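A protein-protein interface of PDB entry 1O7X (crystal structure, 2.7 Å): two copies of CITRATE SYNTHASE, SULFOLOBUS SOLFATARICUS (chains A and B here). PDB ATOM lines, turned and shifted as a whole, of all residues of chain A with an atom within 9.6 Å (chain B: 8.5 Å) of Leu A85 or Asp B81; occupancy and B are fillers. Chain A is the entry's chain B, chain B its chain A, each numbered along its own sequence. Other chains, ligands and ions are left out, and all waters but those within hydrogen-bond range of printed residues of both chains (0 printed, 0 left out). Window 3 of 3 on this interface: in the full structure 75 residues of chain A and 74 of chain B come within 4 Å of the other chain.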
ATOM      1  N   GLN A  77      33.863  -5.763  -4.979  1.00  0.00           N
ATOM      2  CA  GLN A  77      33.832  -7.156  -4.560  1.00  0.00           C
ATOM      3  C   GLN A  77      32.806  -7.939  -5.343  1.00  0.00           C
ATOM      4  O   GLN A  77      33.068  -9.075  -5.724  1.00  0.00           O
ATOM      5  CB  GLN A  77      33.597  -7.289  -3.057  1.00  0.00           C
ATOM      6  CG  GLN A  77      33.420  -8.689  -2.526  1.00  0.00           C
ATOM      7  CD  GLN A  77      34.652  -9.566  -2.556  1.00  0.00           C
ATOM      8  OE1 GLN A  77      35.765  -9.226  -2.978  1.00  0.00           O
ATOM      9  NE2 GLN A  77      34.496 -10.813  -2.092  1.00  0.00           N
ATOM     10  N   GLU A  78      31.677  -7.322  -5.657  1.00  0.00           N
ATOM     11  CA  GLU A  78      30.590  -7.963  -6.397  1.00  0.00           C
ATOM     12  C   GLU A  78      31.047  -8.486  -7.749  1.00  0.00           C
ATOM     13  O   GLU A  78      30.588  -9.547  -8.175  1.00  0.00           O
ATOM     14  CB  GLU A  78      29.417  -6.999  -6.568  1.00  0.00           C
ATOM     15  CG  GLU A  78      29.103  -6.217  -5.316  1.00  0.00           C
ATOM     16  CD  GLU A  78      29.886  -4.934  -5.113  1.00  0.00           C
ATOM     17  OE1 GLU A  78      30.242  -4.165  -6.032  1.00  0.00           O
ATOM     18  OE2 GLU A  78      30.153  -4.659  -3.921  1.00  0.00           O
ATOM     19  N   VAL A  79      31.985  -7.788  -8.389  1.00  0.00           N
ATOM     20  CA  VAL A  79      32.528  -8.295  -9.646  1.00  0.00           C
ATOM     21  C   VAL A  79      33.314  -9.566  -9.359  1.00  0.00           C
ATOM     22  O   VAL A  79      33.194 -10.478 -10.171  1.00  0.00           O
ATOM     23  CB  VAL A  79      33.364  -7.266 -10.419  1.00  0.00           C
ATOM     24  CG1 VAL A  79      33.815  -7.809 -11.758  1.00  0.00           C
ATOM     25  CG2 VAL A  79      32.577  -5.975 -10.648  1.00  0.00           C
ATOM     26  N   LEU A  80      34.028  -9.717  -8.247  1.00  0.00           N
ATOM     27  CA  LEU A  80      34.755 -10.964  -8.037  1.00  0.00           C
ATOM     28  C   LEU A  80      33.798 -12.056  -7.590  1.00  0.00           C
ATOM     29  O   LEU A  80      33.863 -13.187  -8.104  1.00  0.00           O
ATOM     30  CB  LEU A  80      35.971 -10.782  -7.142  1.00  0.00           C
ATOM     31  CG  LEU A  80      37.086  -9.882  -7.705  1.00  0.00           C
ATOM     32  CD1 LEU A  80      37.817  -9.193  -6.570  1.00  0.00           C
ATOM     33  CD2 LEU A  80      38.054 -10.638  -8.593  1.00  0.00           C
ATOM     34  N   ASP A  81      32.807 -11.704  -6.782  1.00  0.00           N
ATOM     35  CA  ASP A  81      31.824 -12.681  -6.353  1.00  0.00           C
ATOM     36  C   ASP A  81      31.076 -13.320  -7.505  1.00  0.00           C
ATOM     37  O   ASP A  81      30.853 -14.541  -7.505  1.00  0.00           O
ATOM     38  CB  ASP A  81      30.894 -12.036  -5.314  1.00  0.00           C
ATOM     39  CG  ASP A  81      31.560 -11.973  -3.937  1.00  0.00           C
ATOM     40  OD1 ASP A  81      32.697 -12.493  -3.804  1.00  0.00           O
ATOM     41  OD2 ASP A  81      30.968 -11.427  -2.972  1.00  0.00           O
ATOM     42  N   THR A  82      30.672 -12.592  -8.539  1.00  0.00           N
ATOM     43  CA  THR A  82      29.948 -13.106  -9.681  1.00  0.00           C
ATOM     44  C   THR A  82      30.759 -14.128 -10.464  1.00  0.00           C
ATOM     45  O   THR A  82      30.214 -15.081 -11.021  1.00  0.00           O
ATOM     46  CB  THR A  82      29.582 -11.980 -10.675  1.00  0.00           C
ATOM     47  OG1 THR A  82      28.865 -10.970  -9.960  1.00  0.00           O
ATOM     48  CG2 THR A  82      28.695 -12.497 -11.794  1.00  0.00           C
ATOM     49  N   ILE A  83      32.060 -13.844 -10.582  1.00  0.00           N
ATOM     50  CA  ILE A  83      32.959 -14.699 -11.359  1.00  0.00           C
ATOM     51  C   ILE A  83      33.072 -16.048 -10.676  1.00  0.00           C
ATOM     52  O   ILE A  83      33.096 -17.100 -11.290  1.00  0.00           O
ATOM     53  CB  ILE A  83      34.288 -13.956 -11.593  1.00  0.00           C
ATOM     54  CG1 ILE A  83      34.134 -13.179 -12.915  1.00  0.00           C
ATOM     55  CG2 ILE A  83      35.519 -14.835 -11.710  1.00  0.00           C
ATOM     56  CD1 ILE A  83      34.987 -11.957 -13.018  1.00  0.00           C
ATOM     57  N   TYR A  84      33.109 -15.995  -9.343  1.00  0.00           N
ATOM     58  CA  TYR A  84      33.207 -17.137  -8.458  1.00  0.00           C
ATOM     59  C   TYR A  84      31.871 -17.862  -8.300  1.00  0.00           C
ATOM     60  O   TYR A  84      31.913 -19.015  -7.851  1.00  0.00           O
ATOM     61  CB  TYR A  84      33.788 -16.743  -7.094  1.00  0.00           C
ATOM     62  CG  TYR A  84      35.299 -16.833  -7.128  1.00  0.00           C
ATOM     63  CD1 TYR A  84      36.031 -15.733  -7.568  1.00  0.00           C
ATOM     64  CD2 TYR A  84      35.996 -17.994  -6.810  1.00  0.00           C
ATOM     65  CE1 TYR A  84      37.412 -15.785  -7.636  1.00  0.00           C
ATOM     66  CE2 TYR A  84      37.361 -18.063  -6.896  1.00  0.00           C
ATOM     67  CZ  TYR A  84      38.068 -16.954  -7.287  1.00  0.00           C
ATOM     68  OH  TYR A  84      39.445 -16.943  -7.372  1.00  0.00           O
ATOM     69  N   LEU A  85      30.752 -17.245  -8.677  1.00  0.00           N
ATOM     70  CA  LEU A  85      29.484 -17.965  -8.688  1.00  0.00           C
ATOM     71  C   LEU A  85      29.437 -18.837  -9.944  1.00  0.00           C
ATOM     72  O   LEU A  85      28.804 -19.887  -9.897  1.00  0.00           O
ATOM     73  CB  LEU A  85      28.292 -17.040  -8.648  1.00  0.00           C
ATOM     74  CG  LEU A  85      27.257 -17.031  -7.536  1.00  0.00           C
ATOM     75  CD1 LEU A  85      27.779 -17.559  -6.211  1.00  0.00           C
ATOM     76  CD2 LEU A  85      26.702 -15.613  -7.351  1.00  0.00           C
ATOM     77  N   MET A  86      30.079 -18.444 -11.045  1.00  0.00           N
ATOM     78  CA  MET A  86      30.055 -19.262 -12.247  1.00  0.00           C
ATOM     79  C   MET A  86      30.886 -20.527 -12.059  1.00  0.00           C
ATOM     80  O   MET A  86      31.806 -20.642 -11.237  1.00  0.00           O
ATOM     81  CB  MET A  86      30.566 -18.539 -13.482  1.00  0.00           C
ATOM     82  CG  MET A  86      29.954 -17.169 -13.685  1.00  0.00           C
ATOM     83  SD  MET A  86      28.146 -17.235 -13.594  1.00  0.00           S
ATOM     84  CE  MET A  86      27.884 -18.078 -15.144  1.00  0.00           C
ATOM     85  N   PRO A  87      30.560 -21.523 -12.867  1.00  0.00           N
ATOM     86  CA  PRO A  87      31.257 -22.792 -12.790  1.00  0.00           C
ATOM     87  C   PRO A  87      32.721 -22.569 -13.073  1.00  0.00           C
ATOM     88  O   PRO A  87      33.145 -21.859 -13.971  1.00  0.00           O
ATOM     89  CB  PRO A  87      30.580 -23.677 -13.819  1.00  0.00           C
ATOM     90  CG  PRO A  87      29.864 -22.753 -14.742  1.00  0.00           C
ATOM     91  CD  PRO A  87      29.524 -21.528 -13.928  1.00  0.00           C
ATOM     92  N   LYS A  88      33.530 -23.299 -12.336  1.00  0.00           N
ATOM     93  CA  LYS A  88      34.984 -23.375 -12.448  1.00  0.00           C
ATOM     94  C   LYS A  88      35.299 -23.875 -13.836  1.00  0.00           C
ATOM     95  O   LYS A  88      36.197 -23.363 -14.502  1.00  0.00           O
ATOM     96  CB  LYS A  88      35.404 -24.364 -11.390  1.00  0.00           C
ATOM     97  CG  LYS A  88      36.799 -24.898 -11.274  1.00  0.00           C
ATOM     98  CD  LYS A  88      36.760 -26.166 -10.445  1.00  0.00           C
ATOM     99  CE  LYS A  88      38.131 -26.659 -10.022  1.00  0.00           C
ATOM    100  NZ  LYS A  88      37.983 -27.668  -8.908  1.00  0.00           N
ATOM    101  N   GLU A  89      34.519 -24.818 -14.347  1.00  0.00           N
ATOM    102  CA  GLU A  89      34.704 -25.375 -15.670  1.00  0.00           C
ATOM    103  C   GLU A  89      34.391 -24.460 -16.840  1.00  0.00           C
ATOM    104  O   GLU A  89      34.694 -24.817 -17.991  1.00  0.00           O
ATOM    105  CB  GLU A  89      33.817 -26.618 -15.780  1.00  0.00           C
ATOM    106  CG  GLU A  89      33.971 -27.537 -14.575  1.00  0.00           C
ATOM    107  CD  GLU A  89      32.994 -27.186 -13.466  1.00  0.00           C
ATOM    108  OE1 GLU A  89      31.809 -26.967 -13.804  1.00  0.00           O
ATOM    109  OE2 GLU A  89      33.430 -27.133 -12.300  1.00  0.00           O
ATOM    110  N   ALA A  90      33.780 -23.309 -16.637  1.00  0.00           N
ATOM    111  CA  ALA A  90      33.425 -22.393 -17.692  1.00  0.00           C
ATOM    112  C   ALA A  90      34.606 -21.854 -18.495  1.00  0.00           C
ATOM    113  O   ALA A  90      35.717 -21.582 -18.086  1.00  0.00           O
ATOM    114  CB  ALA A  90      32.635 -21.250 -17.061  1.00  0.00           C
ATOM    115  N   LEU A  95      33.744 -16.242 -18.859  1.00  0.00           N
ATOM    116  CA  LEU A  95      33.847 -15.582 -17.562  1.00  0.00           C
ATOM    117  C   LEU A  95      34.261 -14.129 -17.709  1.00  0.00           C
ATOM    118  O   LEU A  95      33.817 -13.272 -16.941  1.00  0.00           O
ATOM    119  CB  LEU A  95      34.819 -16.264 -16.592  1.00  0.00           C
ATOM    120  CG  LEU A  95      34.479 -17.707 -16.221  1.00  0.00           C
ATOM    121  CD1 LEU A  95      35.618 -18.341 -15.454  1.00  0.00           C
ATOM    122  CD2 LEU A  95      33.197 -17.803 -15.417  1.00  0.00           C
ATOM    123  N   VAL A  98      31.013 -12.113 -18.413  1.00  0.00           N
ATOM    124  CA  VAL A  98      30.244 -11.867 -17.206  1.00  0.00           C
ATOM    125  C   VAL A  98      30.898 -10.741 -16.398  1.00  0.00           C
ATOM    126  O   VAL A  98      30.217  -9.797 -15.993  1.00  0.00           O
ATOM    127  CB  VAL A  98      30.175 -13.063 -16.233  1.00  0.00           C
ATOM    128  CG1 VAL A  98      29.087 -12.828 -15.185  1.00  0.00           C
ATOM    129  CG2 VAL A  98      29.961 -14.373 -16.969  1.00  0.00           C
ATOM    130  N   ASN A 133      42.239 -13.097 -11.973  1.00  0.00           N
ATOM    131  CA  ASN A 133      41.208 -13.819 -11.267  1.00  0.00           C
ATOM    132  C   ASN A 133      40.366 -14.814 -12.053  1.00  0.00           C
ATOM    133  O   ASN A 133      39.759 -15.732 -11.460  1.00  0.00           O
ATOM    134  CB  ASN A 133      40.362 -12.686 -10.622  1.00  0.00           C
ATOM    135  CG  ASN A 133      41.232 -12.031  -9.551  1.00  0.00           C
ATOM    136  OD1 ASN A 133      41.753 -12.774  -8.719  1.00  0.00           O
ATOM    137  ND2 ASN A 133      41.416 -10.725  -9.549  1.00  0.00           N
ATOM    138  N   ARG A 137      40.331 -18.345 -10.480  1.00  0.00           N
ATOM    139  CA  ARG A 137      39.053 -18.996 -10.221  1.00  0.00           C
ATOM    140  C   ARG A 137      39.002 -20.353 -10.876  1.00  0.00           C
ATOM    141  O   ARG A 137      38.543 -21.277 -10.188  1.00  0.00           O
ATOM    142  CB  ARG A 137      37.935 -18.032 -10.535  1.00  0.00           C
ATOM    143  CG  ARG A 137      36.724 -18.629 -11.219  1.00  0.00           C
ATOM    144  CD  ARG A 137      35.699 -19.044 -10.211  1.00  0.00           C
ATOM    145  NE  ARG A 137      35.035 -20.295 -10.595  1.00  0.00           N
ATOM    146  CZ  ARG A 137      34.502 -21.066  -9.651  1.00  0.00           C
ATOM    147  NH1 ARG A 137      34.555 -20.750  -8.369  1.00  0.00           N
ATOM    148  NH2 ARG A 137      33.880 -22.182  -9.942  1.00  0.00           N
ATOM    149  N   VAL B  75      15.786 -20.925 -14.286  1.00  0.00           N
ATOM    150  CA  VAL B  75      17.149 -20.513 -14.530  1.00  0.00           C
ATOM    151  C   VAL B  75      17.971 -20.876 -13.288  1.00  0.00           C
ATOM    152  O   VAL B  75      17.503 -20.711 -12.157  1.00  0.00           O
ATOM    153  CB  VAL B  75      17.345 -19.027 -14.865  1.00  0.00           C
ATOM    154  CG1 VAL B  75      16.486 -18.604 -16.049  1.00  0.00           C
ATOM    155  CG2 VAL B  75      17.093 -18.077 -13.699  1.00  0.00           C
ATOM    156  N   PRO B  76      19.183 -21.375 -13.481  1.00  0.00           N
ATOM    157  CA  PRO B  76      20.058 -21.705 -12.364  1.00  0.00           C
ATOM    158  C   PRO B  76      20.065 -20.567 -11.355  1.00  0.00           C
ATOM    159  O   PRO B  76      20.010 -19.395 -11.745  1.00  0.00           O
ATOM    160  CB  PRO B  76      21.404 -21.921 -13.033  1.00  0.00           C
ATOM    161  CG  PRO B  76      21.092 -22.323 -14.427  1.00  0.00           C
ATOM    162  CD  PRO B  76      19.830 -21.582 -14.798  1.00  0.00           C
ATOM    163  N   GLN B  77      20.156 -20.847 -10.054  1.00  0.00           N
ATOM    164  CA  GLN B  77      20.138 -19.793  -9.044  1.00  0.00           C
ATOM    165  C   GLN B  77      21.308 -18.823  -9.107  1.00  0.00           C
ATOM    166  O   GLN B  77      21.174 -17.665  -8.678  1.00  0.00           O
ATOM    167  CB  GLN B  77      19.975 -20.386  -7.644  1.00  0.00           C
ATOM    168  CG  GLN B  77      19.915 -19.419  -6.481  1.00  0.00           C
ATOM    169  CD  GLN B  77      18.585 -18.726  -6.285  1.00  0.00           C
ATOM    170  OE1 GLN B  77      17.512 -19.254  -6.615  1.00  0.00           O
ATOM    171  NE2 GLN B  77      18.596 -17.511  -5.724  1.00  0.00           N
ATOM    172  N   GLU B  78      22.417 -19.213  -9.706  1.00  0.00           N
ATOM    173  CA  GLU B  78      23.608 -18.388  -9.847  1.00  0.00           C
ATOM    174  C   GLU B  78      23.308 -17.188 -10.731  1.00  0.00           C
ATOM    175  O   GLU B  78      23.720 -16.092 -10.366  1.00  0.00           O
ATOM    176  CB  GLU B  78      24.799 -19.146 -10.422  1.00  0.00           C
ATOM    177  CG  GLU B  78      25.172 -20.366  -9.601  1.00  0.00           C
ATOM    178  CD  GLU B  78      24.112 -21.453  -9.685  1.00  0.00           C
ATOM    179  OE1 GLU B  78      23.562 -21.615 -10.790  1.00  0.00           O
ATOM    180  OE2 GLU B  78      23.830 -22.085  -8.648  1.00  0.00           O
ATOM    181  N   VAL B  79      22.578 -17.397 -11.816  1.00  0.00           N
ATOM    182  CA  VAL B  79      22.198 -16.258 -12.641  1.00  0.00           C
ATOM    183  C   VAL B  79      21.390 -15.265 -11.794  1.00  0.00           C
ATOM    184  O   VAL B  79      21.725 -14.069 -11.764  1.00  0.00           O
ATOM    185  CB  VAL B  79      21.362 -16.648 -13.865  1.00  0.00           C
ATOM    186  CG1 VAL B  79      21.025 -15.400 -14.667  1.00  0.00           C
ATOM    187  CG2 VAL B  79      22.103 -17.649 -14.727  1.00  0.00           C
ATOM    188  N   LEU B  80      20.383 -15.762 -11.074  1.00  0.00           N
ATOM    189  CA  LEU B  80      19.601 -14.845 -10.262  1.00  0.00           C
ATOM    190  C   LEU B  80      20.480 -14.232  -9.189  1.00  0.00           C
ATOM    191  O   LEU B  80      20.348 -13.014  -9.025  1.00  0.00           O
ATOM    192  CB  LEU B  80      18.326 -15.430  -9.678  1.00  0.00           C
ATOM    193  CG  LEU B  80      17.399 -16.128 -10.680  1.00  0.00           C
ATOM    194  CD1 LEU B  80      16.456 -17.083  -9.966  1.00  0.00           C
ATOM    195  CD2 LEU B  80      16.648 -15.083 -11.489  1.00  0.00           C
ATOM    196  N   ASP B  81      21.378 -14.974  -8.535  1.00  0.00           N
ATOM    197  CA  ASP B  81      22.234 -14.376  -7.520  1.00  0.00           C
ATOM    198  C   ASP B  81      23.086 -13.262  -8.097  1.00  0.00           C
ATOM    199  O   ASP B  81      23.326 -12.219  -7.501  1.00  0.00           O
ATOM    200  CB  ASP B  81      23.159 -15.391  -6.875  1.00  0.00           C
ATOM    201  CG  ASP B  81      22.431 -16.442  -6.061  1.00  0.00           C
ATOM    202  OD1 ASP B  81      21.186 -16.374  -5.920  1.00  0.00           O
ATOM    203  OD2 ASP B  81      23.181 -17.338  -5.589  1.00  0.00           O
ATOM    204  N   THR B  82      23.597 -13.472  -9.286  1.00  0.00           N
ATOM    205  CA  THR B  82      24.391 -12.503 -10.024  1.00  0.00           C
ATOM    206  C   THR B  82      23.613 -11.212 -10.222  1.00  0.00           C
ATOM    207  O   THR B  82      24.132 -10.112 -10.011  1.00  0.00           O
ATOM    208  CB  THR B  82      24.717 -13.206 -11.360  1.00  0.00           C
ATOM    209  OG1 THR B  82      25.912 -13.969 -11.211  1.00  0.00           O
ATOM    210  CG2 THR B  82      24.847 -12.250 -12.512  1.00  0.00           C
ATOM    211  N   ILE B  83      22.352 -11.335 -10.647  1.00  0.00           N
ATOM    212  CA  ILE B  83      21.480 -10.191 -10.914  1.00  0.00           C
ATOM    213  C   ILE B  83      21.217  -9.508  -9.577  1.00  0.00           C
ATOM    214  O   ILE B  83      21.245  -8.285  -9.466  1.00  0.00           O
ATOM    215  CB  ILE B  83      20.165 -10.557 -11.611  1.00  0.00           C
ATOM    216  CG1 ILE B  83      20.391 -10.788 -13.121  1.00  0.00           C
ATOM    217  CG2 ILE B  83      19.066  -9.500 -11.438  1.00  0.00           C
ATOM    218  CD1 ILE B  83      19.173 -11.437 -13.753  1.00  0.00           C
ATOM    219  N   TYR B  84      21.016 -10.306  -8.534  1.00  0.00           N
ATOM    220  CA  TYR B  84      20.786  -9.694  -7.232  1.00  0.00           C
ATOM    221  C   TYR B  84      22.085  -9.164  -6.629  1.00  0.00           C
ATOM    222  O   TYR B  84      21.914  -8.309  -5.733  1.00  0.00           O
ATOM    223  CB  TYR B  84      19.963 -10.608  -6.330  1.00  0.00           C
ATOM    224  CG  TYR B  84      18.464 -10.468  -6.556  1.00  0.00           C
ATOM    225  CD1 TYR B  84      17.854 -10.992  -7.691  1.00  0.00           C
ATOM    226  CD2 TYR B  84      17.674  -9.792  -5.637  1.00  0.00           C
ATOM    227  CE1 TYR B  84      16.499 -10.857  -7.896  1.00  0.00           C
ATOM    228  CE2 TYR B  84      16.309  -9.636  -5.835  1.00  0.00           C
ATOM    229  CZ  TYR B  84      15.726 -10.177  -6.969  1.00  0.00           C
ATOM    230  OH  TYR B  84      14.386 -10.014  -7.177  1.00  0.00           O
ATOM    231  N   LEU B  85      23.289  -9.472  -7.109  1.00  0.00           N
ATOM    232  CA  LEU B  85      24.494  -8.857  -6.612  1.00  0.00           C
ATOM    233  C   LEU B  85      24.743  -7.458  -7.179  1.00  0.00           C
ATOM    234  O   LEU B  85      25.503  -6.691  -6.564  1.00  0.00           O
ATOM    235  CB  LEU B  85      25.765  -9.676  -6.891  1.00  0.00           C
ATOM    236  CG  LEU B  85      25.995 -10.911  -6.025  1.00  0.00           C
ATOM    237  CD1 LEU B  85      27.152 -11.718  -6.589  1.00  0.00           C
ATOM    238  CD2 LEU B  85      26.217 -10.584  -4.552  1.00  0.00           C
ATOM    239  N   MET B  86      24.180  -7.091  -8.327  1.00  0.00           N
ATOM    240  CA  MET B  86      24.369  -5.747  -8.875  1.00  0.00           C
ATOM    241  C   MET B  86      23.487  -4.703  -8.193  1.00  0.00           C
ATOM    242  O   MET B  86      22.469  -4.973  -7.530  1.00  0.00           O
ATOM    243  CB  MET B  86      24.088  -5.832 -10.376  1.00  0.00           C
ATOM    244  CG  MET B  86      24.816  -6.983 -11.067  1.00  0.00           C
ATOM    245  SD  MET B  86      26.617  -6.824 -10.856  1.00  0.00           S
ATOM    246  CE  MET B  86      26.843  -5.330 -11.778  1.00  0.00           C
ATOM    247  N   VAL B  98      24.303  -8.796 -17.942  1.00  0.00           N
ATOM    248  CA  VAL B  98      24.923  -9.638 -16.929  1.00  0.00           C
ATOM    249  C   VAL B  98      24.305 -11.030 -16.909  1.00  0.00           C
ATOM    250  O   VAL B  98      24.972 -12.043 -16.731  1.00  0.00           O
ATOM    251  CB  VAL B  98      24.743  -8.971 -15.559  1.00  0.00           C
ATOM    252  CG1 VAL B  98      25.185  -9.905 -14.465  1.00  0.00           C
ATOM    253  CG2 VAL B  98      25.527  -7.679 -15.477  1.00  0.00           C
ATOM    254  N   ALA B 102      25.909 -14.445 -17.801  1.00  0.00           N
ATOM    255  CA  ALA B 102      25.998 -15.553 -16.821  1.00  0.00           C
ATOM    256  C   ALA B 102      25.530 -16.824 -17.504  1.00  0.00           C
ATOM    257  O   ALA B 102      26.353 -17.723 -17.668  1.00  0.00           O
ATOM    258  CB  ALA B 102      25.430 -15.223 -15.468  1.00  0.00           C
ATOM    259  N   SER B 105      28.101 -18.555 -20.049  1.00  0.00           N
ATOM    260  CA  SER B 105      29.240 -19.274 -19.499  1.00  0.00           C
ATOM    261  C   SER B 105      28.810 -20.502 -18.733  1.00  0.00           C
ATOM    262  O   SER B 105      29.647 -21.403 -18.638  1.00  0.00           O
ATOM    263  CB  SER B 105      30.180 -18.342 -18.756  1.00  0.00           C
ATOM    264  OG  SER B 105      29.706 -17.917 -17.507  1.00  0.00           O
ATOM    265  N   ILE B 106      27.583 -20.671 -18.319  1.00  0.00           N
ATOM    266  CA  ILE B 106      27.134 -21.887 -17.652  1.00  0.00           C
ATOM    267  C   ILE B 106      26.775 -22.960 -18.671  1.00  0.00           C
ATOM    268  O   ILE B 106      26.761 -24.154 -18.392  1.00  0.00           O
ATOM    269  CB  ILE B 106      25.885 -21.576 -16.793  1.00  0.00           C
ATOM    270  CG1 ILE B 106      26.274 -20.937 -15.456  1.00  0.00           C
ATOM    271  CG2 ILE B 106      25.027 -22.789 -16.537  1.00  0.00           C
ATOM    272  CD1 ILE B 106      25.141 -20.246 -14.735  1.00  0.00           C
ATOM    273  N   ASN B 133      12.678 -10.993 -13.487  1.00  0.00           N
ATOM    274  CA  ASN B 133      13.529 -10.775 -12.313  1.00  0.00           C
ATOM    275  C   ASN B 133      14.412  -9.560 -12.298  1.00  0.00           C
ATOM    276  O   ASN B 133      14.779  -9.084 -11.221  1.00  0.00           O
ATOM    277  CB  ASN B 133      14.304 -12.063 -12.025  1.00  0.00           C
ATOM    278  CG  ASN B 133      13.238 -13.053 -11.547  1.00  0.00           C
ATOM    279  OD1 ASN B 133      12.736 -12.841 -10.443  1.00  0.00           O
ATOM    280  ND2 ASN B 133      12.923 -14.025 -12.382  1.00  0.00           N
ATOM    281  N   ARG B 137      14.118  -7.137  -8.947  1.00  0.00           N
ATOM    282  CA  ARG B 137      15.315  -6.676  -8.261  1.00  0.00           C
ATOM    283  C   ARG B 137      15.414  -5.171  -8.231  1.00  0.00           C
ATOM    284  O   ARG B 137      16.058  -4.628  -7.330  1.00  0.00           O
ATOM    285  CB  ARG B 137      16.523  -7.330  -8.927  1.00  0.00           C
ATOM    286  CG  ARG B 137      17.691  -6.421  -9.243  1.00  0.00           C
ATOM    287  CD  ARG B 137      18.864  -6.702  -8.346  1.00  0.00           C
ATOM    288  NE  ARG B 137      19.405  -5.494  -7.730  1.00  0.00           N
ATOM    289  CZ  ARG B 137      19.480  -5.372  -6.412  1.00  0.00           C
ATOM    290  NH1 ARG B 137      19.061  -6.341  -5.625  1.00  0.00           N
ATOM    291  NH2 ARG B 137      19.958  -4.320  -5.803  1.00  0.00           N
ATOM    292  N   PRO B 143      13.009 -12.840  -5.892  1.00  0.00           N
ATOM    293  CA  PRO B 143      12.902 -13.361  -7.231  1.00  0.00           C
ATOM    294  C   PRO B 143      11.737 -14.316  -7.423  1.00  0.00           C
ATOM    295  O   PRO B 143      11.432 -15.081  -6.514  1.00  0.00           O
ATOM    296  CB  PRO B 143      14.220 -14.078  -7.478  1.00  0.00           C
ATOM    297  CG  PRO B 143      14.808 -14.326  -6.140  1.00  0.00           C
ATOM    298  CD  PRO B 143      14.260 -13.272  -5.232  1.00  0.00           C
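Glu A78 touches Leu B85 (CG to O, 3.8 Å). Asp A81 touches Leu B85. CG2 of Thr A82 touches OG1 of Thr B82, 3.2 Å away. Thr A82 touches Leu B85. O of Leu A85 touches CG of Glu B78, at 3.7 Å. Asp B81 touches Leu A85 (CB to CD2, 3.6 Å). CD2 of Leu A85 touches CD1 of Leu B85, at 3.99 Å. Pro A87 touches Ile B106. Ser B105 touches Ala A90 (O to CB, 3.4 Å). Ser B105 touches Val A98 (OG to CG2, 3.6 Å).
OG of Ser B105 is in hydrogen-bond range of O of Ala B102 (3.4 Å). O of Glu B78 is in hydrogen-bond range of OG1 of Thr B82 (3.2 Å). O of Met A86 is in hydrogen-bond range of NH2 of Arg A137, 2.9 Å away. The side-chain amide nitrogen (NE2) of Gln A77 sits at hydrogen-bond distance from the side-chain carboxylate (OD1) of Asp A81 (3.0 Å). The side-chain amide nitrogen (NE2) of Gln B77 lies within hydrogen-bond range of the side-chain carboxylate (OD1) of Asp B81 (2.8 Å). The backbone carbonyl oxygen (O) of Glu A78 sits at hydrogen-bond distance from the side-chain hydroxyl (OG1) of Thr A82, 2.9 Å away.
Glu A78 touches Leu B85, and with the chains exchanged Leu A85 touches Glu B78. Asp A81 touches Leu B85, and with the chains exchanged Leu A85 touches Asp B81. Thr A82 touches Leu B85, but with the chains exchanged Leu A85 does not touch Thr B82 (4.2 Å). Leu B85 touches its own counterpart, Leu A85. 13 positions are printed for both chains.
Printed residues of chain B within 4 Å of Asp A81: Leu B85. Of the printed residues of chain B, Thr A82 touches Thr B82 and Leu B85. Of the printed residues of chain B, Leu A85 touches Glu B78, Asp B81 and Leu B85. Thr B82 touches just one residue of chain A: Thr A82. The nearest residue of chain A that does not touch Asp B81 is Thr A82 (6.2 Å).
Of the 18 printed residues of chain A, 8 touch a printed residue of chain B. Hydrophobic or aromatic side chains of chain A within 4 Å of the printed part of chain B: Leu A85, Met A86, Pro A87, Ala A90 and Val A98. Printed residues of chain B that touch a printed residue of chain A: Glu B78, Asp B81, Thr B82, Leu B85, Ala B102, Ser B105 and Ile B106. Hydrophobic or aromatic side chains of chain B within 4 Å of the printed part of chain A: Leu B85, Ala B102 and Ile B106. Along chain B the printed residues that touch a printed residue of chain A span positions 78 to 106. Among the printed residues, no Asp or Glu carboxylate lies within 4 Å of a Lys or Arg side-chain nitrogen of the other chain.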
